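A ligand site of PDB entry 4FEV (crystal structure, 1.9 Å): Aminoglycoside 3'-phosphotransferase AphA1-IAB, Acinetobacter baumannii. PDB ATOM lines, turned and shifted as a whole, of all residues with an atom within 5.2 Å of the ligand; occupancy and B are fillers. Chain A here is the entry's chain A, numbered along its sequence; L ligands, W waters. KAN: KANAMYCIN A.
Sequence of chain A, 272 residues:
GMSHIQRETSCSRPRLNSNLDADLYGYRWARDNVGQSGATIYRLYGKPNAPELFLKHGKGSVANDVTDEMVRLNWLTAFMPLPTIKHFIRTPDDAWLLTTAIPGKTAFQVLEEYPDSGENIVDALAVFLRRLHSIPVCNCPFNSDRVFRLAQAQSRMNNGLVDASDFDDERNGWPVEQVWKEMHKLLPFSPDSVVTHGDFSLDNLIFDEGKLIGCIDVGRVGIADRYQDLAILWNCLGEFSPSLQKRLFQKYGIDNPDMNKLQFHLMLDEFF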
ATOM      1  N   GLN A  36      25.734   8.399 -12.860  1.00  0.00           N
ATOM      2  CA  GLN A  36      25.335   7.841 -11.569  1.00  0.00           C
ATOM      3  C   GLN A  36      24.167   6.867 -11.717  1.00  0.00           C
ATOM      4  O   GLN A  36      23.340   6.994 -12.636  1.00  0.00           O
ATOM      5  CB  GLN A  36      25.025   8.941 -10.552  1.00  0.00           C
ATOM      6  CG  GLN A  36      24.802   8.455  -9.108  1.00  0.00           C
ATOM      7  CD  GLN A  36      26.017   7.770  -8.503  1.00  0.00           C
ATOM      8  OE1 GLN A  36      26.292   6.599  -8.764  1.00  0.00           O
ATOM      9  NE2 GLN A  36      26.749   8.508  -7.672  1.00  0.00           N
ATOM     10  N   SER A  37      24.115   5.893 -10.815  1.00  0.00           N
ATOM     11  CA  SER A  37      23.085   4.865 -10.824  1.00  0.00           C
ATOM     12  C   SER A  37      21.721   5.414 -10.372  1.00  0.00           C
ATOM     13  O   SER A  37      21.629   6.509  -9.807  1.00  0.00           O
ATOM     14  CB  SER A  37      23.492   3.710  -9.906  1.00  0.00           C
ATOM     15  OG  SER A  37      23.435   4.101  -8.544  1.00  0.00           O
ATOM     16  N   ARG A 156      20.528  -6.826  -1.784  1.00  0.00           N
ATOM     17  CA  ARG A 156      21.352  -6.248  -2.860  1.00  0.00           C
ATOM     18  C   ARG A 156      22.568  -7.089  -3.178  1.00  0.00           C
ATOM     19  O   ARG A 156      22.919  -7.286  -4.365  1.00  0.00           O
ATOM     20  CB  ARG A 156      21.749  -4.802  -2.533  1.00  0.00           C
ATOM     21  CG  ARG A 156      20.603  -3.829  -2.768  1.00  0.00           C
ATOM     22  CD  ARG A 156      21.009  -2.382  -2.531  1.00  0.00           C
ATOM     23  NE  ARG A 156      22.246  -2.021  -3.218  1.00  0.00           N
ATOM     24  CZ  ARG A 156      22.322  -1.560  -4.459  1.00  0.00           C
ATOM     25  NH1 ARG A 156      23.507  -1.249  -4.963  1.00  0.00           N
ATOM     26  NH2 ARG A 156      21.227  -1.403  -5.185  1.00  0.00           N
ATOM     27  N   ASP A 163      28.145  -2.588  -5.968  1.00  0.00           N
ATOM     28  CA  ASP A 163      29.256  -2.099  -6.784  1.00  0.00           C
ATOM     29  C   ASP A 163      30.578  -2.281  -6.043  1.00  0.00           C
ATOM     30  O   ASP A 163      31.017  -1.410  -5.297  1.00  0.00           O
ATOM     31  CB  ASP A 163      29.043  -0.624  -7.164  1.00  0.00           C
ATOM     32  CG  ASP A 163      30.079  -0.121  -8.171  1.00  0.00           C
ATOM     33  OD1 ASP A 163      31.061  -0.841  -8.449  1.00  0.00           O
ATOM     34  OD2 ASP A 163      29.906   1.005  -8.686  1.00  0.00           O
ATOM     35  N   ASP A 166      33.478   0.304  -6.002  1.00  0.00           N
ATOM     36  CA  ASP A 166      33.265   1.610  -5.400  1.00  0.00           C
ATOM     37  C   ASP A 166      33.472   1.561  -3.886  1.00  0.00           C
ATOM     38  O   ASP A 166      33.080   2.480  -3.163  1.00  0.00           O
ATOM     39  CB  ASP A 166      31.868   2.145  -5.754  1.00  0.00           C
ATOM     40  CG  ASP A 166      31.708   3.657  -5.522  1.00  0.00           C
ATOM     41  OD1 ASP A 166      32.694   4.415  -5.664  1.00  0.00           O
ATOM     42  OD2 ASP A 166      30.578   4.086  -5.221  1.00  0.00           O
ATOM     43  N   PHE A 167      34.102   0.491  -3.397  1.00  0.00           N
ATOM     44  CA  PHE A 167      34.395   0.382  -1.967  1.00  0.00           C
ATOM     45  C   PHE A 167      35.401   1.459  -1.514  1.00  0.00           C
ATOM     46  O   PHE A 167      36.173   1.970  -2.331  1.00  0.00           O
ATOM     47  CB  PHE A 167      34.927  -1.017  -1.599  1.00  0.00           C
ATOM     48  CG  PHE A 167      33.904  -2.115  -1.735  1.00  0.00           C
ATOM     49  CD1 PHE A 167      32.554  -1.822  -1.848  1.00  0.00           C
ATOM     50  CD2 PHE A 167      34.300  -3.455  -1.727  1.00  0.00           C
ATOM     51  CE1 PHE A 167      31.610  -2.858  -1.975  1.00  0.00           C
ATOM     52  CE2 PHE A 167      33.366  -4.472  -1.849  1.00  0.00           C
ATOM     53  CZ  PHE A 167      32.021  -4.173  -1.973  1.00  0.00           C
ATOM     54  N   ASP A 168      35.358   1.796  -0.225  1.00  0.00           N
ATOM     55  CA  ASP A 168      36.328   2.730   0.352  1.00  0.00           C
ATOM     56  C   ASP A 168      37.740   2.138   0.236  1.00  0.00           C
ATOM     57  O   ASP A 168      37.899   0.923   0.105  1.00  0.00           O
ATOM     58  CB  ASP A 168      36.009   3.030   1.813  1.00  0.00           C
ATOM     59  CG  ASP A 168      34.686   3.821   1.996  1.00  0.00           C
ATOM     60  OD1 ASP A 168      34.366   4.669   1.140  1.00  0.00           O
ATOM     61  OD2 ASP A 168      33.983   3.591   3.005  1.00  0.00           O
ATOM     62  N   ASP A 169      38.765   2.980   0.318  1.00  0.00           N
ATOM     63  CA  ASP A 169      40.149   2.530   0.107  1.00  0.00           C
ATOM     64  C   ASP A 169      40.552   1.362   1.008  1.00  0.00           C
ATOM     65  O   ASP A 169      41.231   0.447   0.558  1.00  0.00           O
ATOM     66  CB  ASP A 169      41.129   3.691   0.273  1.00  0.00           C
ATOM     67  CG  ASP A 169      41.104   4.641  -0.900  1.00  0.00           C
ATOM     68  OD1 ASP A 169      40.691   4.229  -2.001  1.00  0.00           O
ATOM     69  OD2 ASP A 169      41.502   5.814  -0.722  1.00  0.00           O
ATOM     70  N   ASP A 199      21.429   9.549   3.322  1.00  0.00           N
ATOM     71  CA  ASP A 199      22.559   9.709   2.379  1.00  0.00           C
ATOM     72  C   ASP A 199      23.124  11.109   2.503  1.00  0.00           C
ATOM     73  O   ASP A 199      23.115  11.895   1.553  1.00  0.00           O
ATOM     74  CB  ASP A 199      22.124   9.412   0.933  1.00  0.00           C
ATOM     75  CG  ASP A 199      23.307   9.158  -0.001  1.00  0.00           C
ATOM     76  OD1 ASP A 199      24.468   9.084   0.480  1.00  0.00           O
ATOM     77  OD2 ASP A 199      23.081   9.030  -1.221  1.00  0.00           O
ATOM     78  N   SER A 201      25.561  13.093   2.252  1.00  0.00           N
ATOM     79  CA  SER A 201      26.860  13.324   1.613  1.00  0.00           C
ATOM     80  C   SER A 201      26.991  14.784   1.222  1.00  0.00           C
ATOM     81  O   SER A 201      26.014  15.546   1.249  1.00  0.00           O
ATOM     82  CB  SER A 201      26.972  12.470   0.356  1.00  0.00           C
ATOM     83  OG  SER A 201      26.069  12.960  -0.626  1.00  0.00           O
ATOM     84  N   ASP A 203      27.239  15.866  -1.649  1.00  0.00           N
ATOM     85  CA  ASP A 203      26.481  16.080  -2.887  1.00  0.00           C
ATOM     86  C   ASP A 203      25.015  16.448  -2.645  1.00  0.00           C
ATOM     87  O   ASP A 203      24.333  16.950  -3.553  1.00  0.00           O
ATOM     88  CB  ASP A 203      26.494  14.822  -3.762  1.00  0.00           C
ATOM     89  CG  ASP A 203      27.878  14.485  -4.293  1.00  0.00           C
ATOM     90  OD1 ASP A 203      28.665  15.420  -4.565  1.00  0.00           O
ATOM     91  OD2 ASP A 203      28.173  13.284  -4.457  1.00  0.00           O
ATOM     92  N   ASN A 204      24.511  16.169  -1.447  1.00  0.00           N
ATOM     93  CA  ASN A 204      23.059  16.253  -1.181  1.00  0.00           C
ATOM     94  C   ASN A 204      22.638  17.440  -0.300  1.00  0.00           C
ATOM     95  O   ASN A 204      21.478  17.527   0.137  1.00  0.00           O
ATOM     96  CB  ASN A 204      22.571  14.941  -0.578  1.00  0.00           C
ATOM     97  CG  ASN A 204      22.571  13.807  -1.601  1.00  0.00           C
ATOM     98  OD1 ASN A 204      22.527  14.067  -2.795  1.00  0.00           O
ATOM     99  ND2 ASN A 204      22.618  12.552  -1.134  1.00  0.00           N
ATOM    100  N   ASP A 217      17.536  14.489  -2.220  1.00  0.00           N
ATOM    101  CA  ASP A 217      17.746  13.048  -2.289  1.00  0.00           C
ATOM    102  C   ASP A 217      17.396  12.319  -0.978  1.00  0.00           C
ATOM    103  O   ASP A 217      18.250  11.684  -0.360  1.00  0.00           O
ATOM    104  CB  ASP A 217      19.179  12.722  -2.715  1.00  0.00           C
ATOM    105  CG  ASP A 217      19.245  11.591  -3.706  1.00  0.00           C
ATOM    106  OD1 ASP A 217      18.888  11.826  -4.877  1.00  0.00           O
ATOM    107  OD2 ASP A 217      19.671  10.479  -3.317  1.00  0.00           O
ATOM    108  N   ARG A 220      15.972   7.736   1.498  1.00  0.00           N
ATOM    109  CA  ARG A 220      16.340   6.837   2.598  1.00  0.00           C
ATOM    110  C   ARG A 220      15.996   7.419   3.977  1.00  0.00           C
ATOM    111  O   ARG A 220      16.340   6.845   5.019  1.00  0.00           O
ATOM    112  CB  ARG A 220      17.832   6.495   2.518  1.00  0.00           C
ATOM    113  CG  ARG A 220      18.207   5.862   1.170  1.00  0.00           C
ATOM    114  CD  ARG A 220      19.682   5.416   1.029  1.00  0.00           C
ATOM    115  NE  ARG A 220      19.852   4.651  -0.207  1.00  0.00           N
ATOM    116  CZ  ARG A 220      20.865   4.793  -1.067  1.00  0.00           C
ATOM    117  NH1 ARG A 220      20.900   4.049  -2.166  1.00  0.00           N
ATOM    118  NH2 ARG A 220      21.837   5.670  -0.854  1.00  0.00           N
ATOM    119  N   ASN A 235      33.027  10.513   6.062  1.00  0.00           N
ATOM    120  CA  ASN A 235      33.748   9.864   4.960  1.00  0.00           C
ATOM    121  C   ASN A 235      33.992  10.843   3.823  1.00  0.00           C
ATOM    122  O   ASN A 235      35.108  10.932   3.293  1.00  0.00           O
ATOM    123  CB  ASN A 235      32.956   8.645   4.464  1.00  0.00           C
ATOM    124  CG  ASN A 235      33.784   7.708   3.599  1.00  0.00           C
ATOM    125  OD1 ASN A 235      34.965   7.477   3.863  1.00  0.00           O
ATOM    126  ND2 ASN A 235      33.167   7.176   2.566  1.00  0.00           N
ATOM    127  N   CYS A 236      32.967  11.599   3.437  1.00  0.00           N
ATOM    128  CA  CYS A 236      33.115  12.609   2.375  1.00  0.00           C
ATOM    129  C   CYS A 236      34.175  13.652   2.698  1.00  0.00           C
ATOM    130  O   CYS A 236      34.948  14.061   1.838  1.00  0.00           O
ATOM    131  CB  CYS A 236      31.805  13.333   2.108  1.00  0.00           C
ATOM    132  SG  CYS A 236      30.519  12.320   1.378  1.00  0.00           S
ATOM    133  N   GLU A 239      38.027  13.222   2.030  1.00  0.00           N
ATOM    134  CA  GLU A 239      38.644  13.532   0.747  1.00  0.00           C
ATOM    135  C   GLU A 239      39.424  14.835   0.850  1.00  0.00           C
ATOM    136  O   GLU A 239      40.348  15.058   0.077  1.00  0.00           O
ATOM    137  CB  GLU A 239      37.584  13.696  -0.338  1.00  0.00           C
ATOM    138  CG  GLU A 239      37.331  12.455  -1.164  1.00  0.00           C
ATOM    139  CD  GLU A 239      36.916  12.789  -2.586  1.00  0.00           C
ATOM    140  OE1 GLU A 239      37.735  12.598  -3.510  1.00  0.00           O
ATOM    141  OE2 GLU A 239      35.761  13.229  -2.773  1.00  0.00           O
ATOM    142  N   ASP A 269      27.183   1.225   4.033  1.00  0.00           N
ATOM    143  CA  ASP A 269      26.922   2.035   2.859  1.00  0.00           C
ATOM    144  C   ASP A 269      27.626   1.454   1.630  1.00  0.00           C
ATOM    145  O   ASP A 269      27.297   1.830   0.510  1.00  0.00           O
ATOM    146  CB  ASP A 269      27.373   3.481   3.074  1.00  0.00           C
ATOM    147  CG  ASP A 269      26.721   4.454   2.086  1.00  0.00           C
ATOM    148  OD1 ASP A 269      25.493   4.350   1.860  1.00  0.00           O
ATOM    149  OD2 ASP A 269      27.446   5.323   1.536  1.00  0.00           O
ATOM    150  N   GLU A 270      28.584   0.549   1.830  1.00  0.00           N
ATOM    151  CA  GLU A 270      29.260  -0.124   0.712  1.00  0.00           C
ATOM    152  C   GLU A 270      28.270  -0.922  -0.140  1.00  0.00           C
ATOM    153  O   GLU A 270      28.524  -1.167  -1.318  1.00  0.00           O
ATOM    154  CB  GLU A 270      30.373  -1.066   1.189  1.00  0.00           C
ATOM    155  CG  GLU A 270      31.508  -0.417   2.014  1.00  0.00           C
ATOM    156  CD  GLU A 270      32.418   0.495   1.202  1.00  0.00           C
ATOM    157  OE1 GLU A 270      31.924   1.236   0.323  1.00  0.00           O
ATOM    158  OE2 GLU A 270      33.647   0.471   1.457  1.00  0.00           O
ATOM    159  N   PHE A 272      25.263  -0.078  -0.967  1.00  0.00           N
ATOM    160  CA  PHE A 272      24.225   0.759  -1.549  1.00  0.00           C
ATOM    161  C   PHE A 272      24.719   1.644  -2.671  1.00  0.00           C
ATOM    162  O   PHE A 272      23.922   2.317  -3.320  1.00  0.00           O
ATOM    163  CB  PHE A 272      23.512   1.564  -0.440  1.00  0.00           C
ATOM    164  CG  PHE A 272      22.742   0.702   0.505  1.00  0.00           C
ATOM    165  CD1 PHE A 272      21.477   0.250   0.169  1.00  0.00           C
ATOM    166  CD2 PHE A 272      23.297   0.291   1.720  1.00  0.00           C
ATOM    167  CE1 PHE A 272      20.757  -0.573   1.037  1.00  0.00           C
ATOM    168  CE2 PHE A 272      22.605  -0.536   2.573  1.00  0.00           C
ATOM    169  CZ  PHE A 272      21.318  -0.969   2.245  1.00  0.00           C
ATOM    170  OXT PHE A 272      25.923   1.674  -2.967  1.00  0.00           O
HETATM  171  C1  KAN L   1      27.611   6.735  -3.964  1.00  0.00           C
HETATM  172  C2  KAN L   1      26.602   7.882  -3.849  1.00  0.00           C
HETATM  173  C3  KAN L   1      25.235   7.380  -3.423  1.00  0.00           C
HETATM  174  C4  KAN L   1      24.749   6.382  -4.438  1.00  0.00           C
HETATM  175  C5  KAN L   1      25.737   5.238  -4.493  1.00  0.00           C
HETATM  176  C6  KAN L   1      25.134   4.291  -5.536  1.00  0.00           C
HETATM  177  C7  KAN L   1      31.151   4.383  -0.769  1.00  0.00           C
HETATM  178  C8  KAN L   1      31.413   5.425  -1.832  1.00  0.00           C
HETATM  179  C9  KAN L   1      30.109   6.233  -2.044  1.00  0.00           C
HETATM  180  C10 KAN L   1      28.933   5.329  -2.495  1.00  0.00           C
HETATM  181  C11 KAN L   1      28.692   4.310  -1.368  1.00  0.00           C
HETATM  182  C12 KAN L   1      29.969   3.490  -1.174  1.00  0.00           C
HETATM  183  C13 KAN L   1      33.294   6.896  -2.430  1.00  0.00           C
HETATM  184  C14 KAN L   1      34.717   7.006  -1.862  1.00  0.00           C
HETATM  185  C15 KAN L   1      34.782   7.883  -0.615  1.00  0.00           C
HETATM  186  C16 KAN L   1      34.287   9.263  -1.035  1.00  0.00           C
HETATM  187  C17 KAN L   1      32.860   9.123  -1.544  1.00  0.00           C
HETATM  188  C18 KAN L   1      32.293  10.467  -1.999  1.00  0.00           C
HETATM  189  N1  KAN L   1      26.016   3.126  -5.650  1.00  0.00           N
HETATM  190  N2  KAN L   1      27.623   3.423  -1.812  1.00  0.00           N
HETATM  191  N3  KAN L   1      32.392   3.584  -0.633  1.00  0.00           N
HETATM  192  N4  KAN L   1      36.169   8.005  -0.133  1.00  0.00           N
HETATM  193  O5  KAN L   1      27.062   5.753  -4.879  1.00  0.00           O
HETATM  194  O6  KAN L   1      27.060   8.833  -2.871  1.00  0.00           O
HETATM  195  O7  KAN L   1      24.320   8.485  -3.363  1.00  0.00           O
HETATM  196  O8  KAN L   1      23.461   5.899  -4.053  1.00  0.00           O
HETATM  197  O9  KAN L   1      27.737   6.093  -2.672  1.00  0.00           O
HETATM  198  O10 KAN L   1      30.361   7.263  -3.022  1.00  0.00           O
HETATM  199  O11 KAN L   1      32.543   6.210  -1.411  1.00  0.00           O
HETATM  200  O12 KAN L   1      32.829   8.222  -2.685  1.00  0.00           O
HETATM  201  O13 KAN L   1      35.151   5.662  -1.614  1.00  0.00           O
HETATM  202  O14 KAN L   1      34.409  10.205   0.023  1.00  0.00           O
HETATM  203  O15 KAN L   1      30.938  10.243  -2.440  1.00  0.00           O
HETATM  204  O   HOH W   1      25.826  11.222  -2.417  1.00  0.00           O
HETATM  205  O   HOH W   2      38.505   9.699  -0.408  1.00  0.00           O
HETATM  206  O   HOH W   3      35.227   4.755  -4.610  1.00  0.00           O
HETATM  207  O   HOH W   4      29.304   9.924  -4.909  1.00  0.00           O
HETATM  208  O   HOH W   5      26.787   7.689  -0.009  1.00  0.00           O
HETATM  209  O   HOH W   6      21.087   5.534  -5.924  1.00  0.00           O
HETATM  210  O   HOH W   7      31.576   6.849  -5.623  1.00  0.00           O
HETATM  211  O   HOH W   8      29.240   9.467  -0.022  1.00  0.00           O
HETATM  212  O   HOH W   9      34.836   9.755  -4.604  1.00  0.00           O
HETATM  213  O   HOH W  10      23.969  11.222  -4.644  1.00  0.00           O
HETATM  214  O   HOH W  11      28.207   3.097  -6.854  1.00  0.00           O
HETATM  215  O   HOH W  12      25.356   4.802  -0.912  1.00  0.00           O
HETATM  216  O   HOH W  13      29.271   5.682  -6.965  1.00  0.00           O
HETATM  217  O   HOH W  14      25.446   0.615  -7.226  1.00  0.00           O
HETATM  218  O   HOH W  15      38.309   5.814   0.570  1.00  0.00           O
HETATM  219  O   HOH W  16      28.419   2.050  -4.182  1.00  0.00           O
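ND2 of Asn 235 is in hydrogen-bond range of OD1 of Asp 168, 3.1 Å away. The side-chain amide nitrogen (ND2) of Asn 204 lies within hydrogen-bond range of the backbone carbonyl oxygen (O) of Asp 199 (2.8 Å). OE2 of Glu 270 is in hydrogen-bond range of N of Asp 168, 2.7 Å away. The guanidinium group of Arg 156 lies within salt-bridge range of the chain-end carboxylate of Phe 272 (3.9 Å). O of Phe 272 is in salt-bridge range of NH1 of Arg 220. The side-chain carboxylate of Asp 199 lies within salt-bridge range of the guanidinium group of Arg 220, 3.6 Å away.
Merely in contact with the ligand: Gln 36 (3.9 Å), Ser 37 (3.5 Å), Phe 167 (3.8 Å), Arg 220 (3.6 Å), Cys 236 (3.6 Å) and Glu 239 (3.9 Å). Of the 20 residues printed, 13 come within 4 Å of the ligand.
The side-chain carboxylate (OD2) of Asp 199 is in hydrogen-bond range of an oxygen (O7) of the ligand. O14 of the ligand is in hydrogen-bond range of O of Asn 235, 3.4 Å away. A nitrogen (N3) of the ligand sits at hydrogen-bond distance from the backbone carbonyl oxygen of Asp 166 (2.8 Å). The side-chain carboxylate (OE1) of Glu 270 lies within salt-bridge range of a nitrogen (N3) of the ligand, 2.6 Å away. A nitrogen (N2) of the ligand lies within salt-bridge range of the chain-end carboxylate (OXT) of Phe 272. A nitrogen (N3) of the ligand is in salt-bridge range of the side-chain carboxylate (OD1) of Asp 168. N2 of the ligand is in hydrogen-bond range of O of Asp 269 (2.8 Å). N2 of the ligand is in salt-bridge range of OD2 of Asp 269 (3.9 Å). N3 of the ligand sits close to N of Asp 168.
Water W11 lies within hydrogen-bond range of a nitrogen (N1) of the ligand (2.5 Å), the side-chain carboxylate (OD2) of Asp 166 (3.0 Å) and the side-chain carboxylate (OD2) of Asp 163 (3.3 Å). Water W12 lies within hydrogen-bond range of N2 of the ligand (2.8 Å) and OD1 of Asp 269 (2.8 Å). Water W7 lies within hydrogen-bond range of OD1 of Asp 166 (2.7 Å) and O10 of the ligand (2.9 Å). Water W13 lies within hydrogen-bond range of OD2 of Asp 166 (2.7 Å) and O5 of the ligand (3.0 Å). Water W3 lies within hydrogen-bond range of the side-chain carboxylate of Asp 166 (2.8 Å) and an oxygen (O13) of the ligand (3.1 Å). Water W15 lies within hydrogen-bond range of the backbone NH of Asp 169 (2.9 Å) and a nitrogen (N4) of the ligand (3.1 Å).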
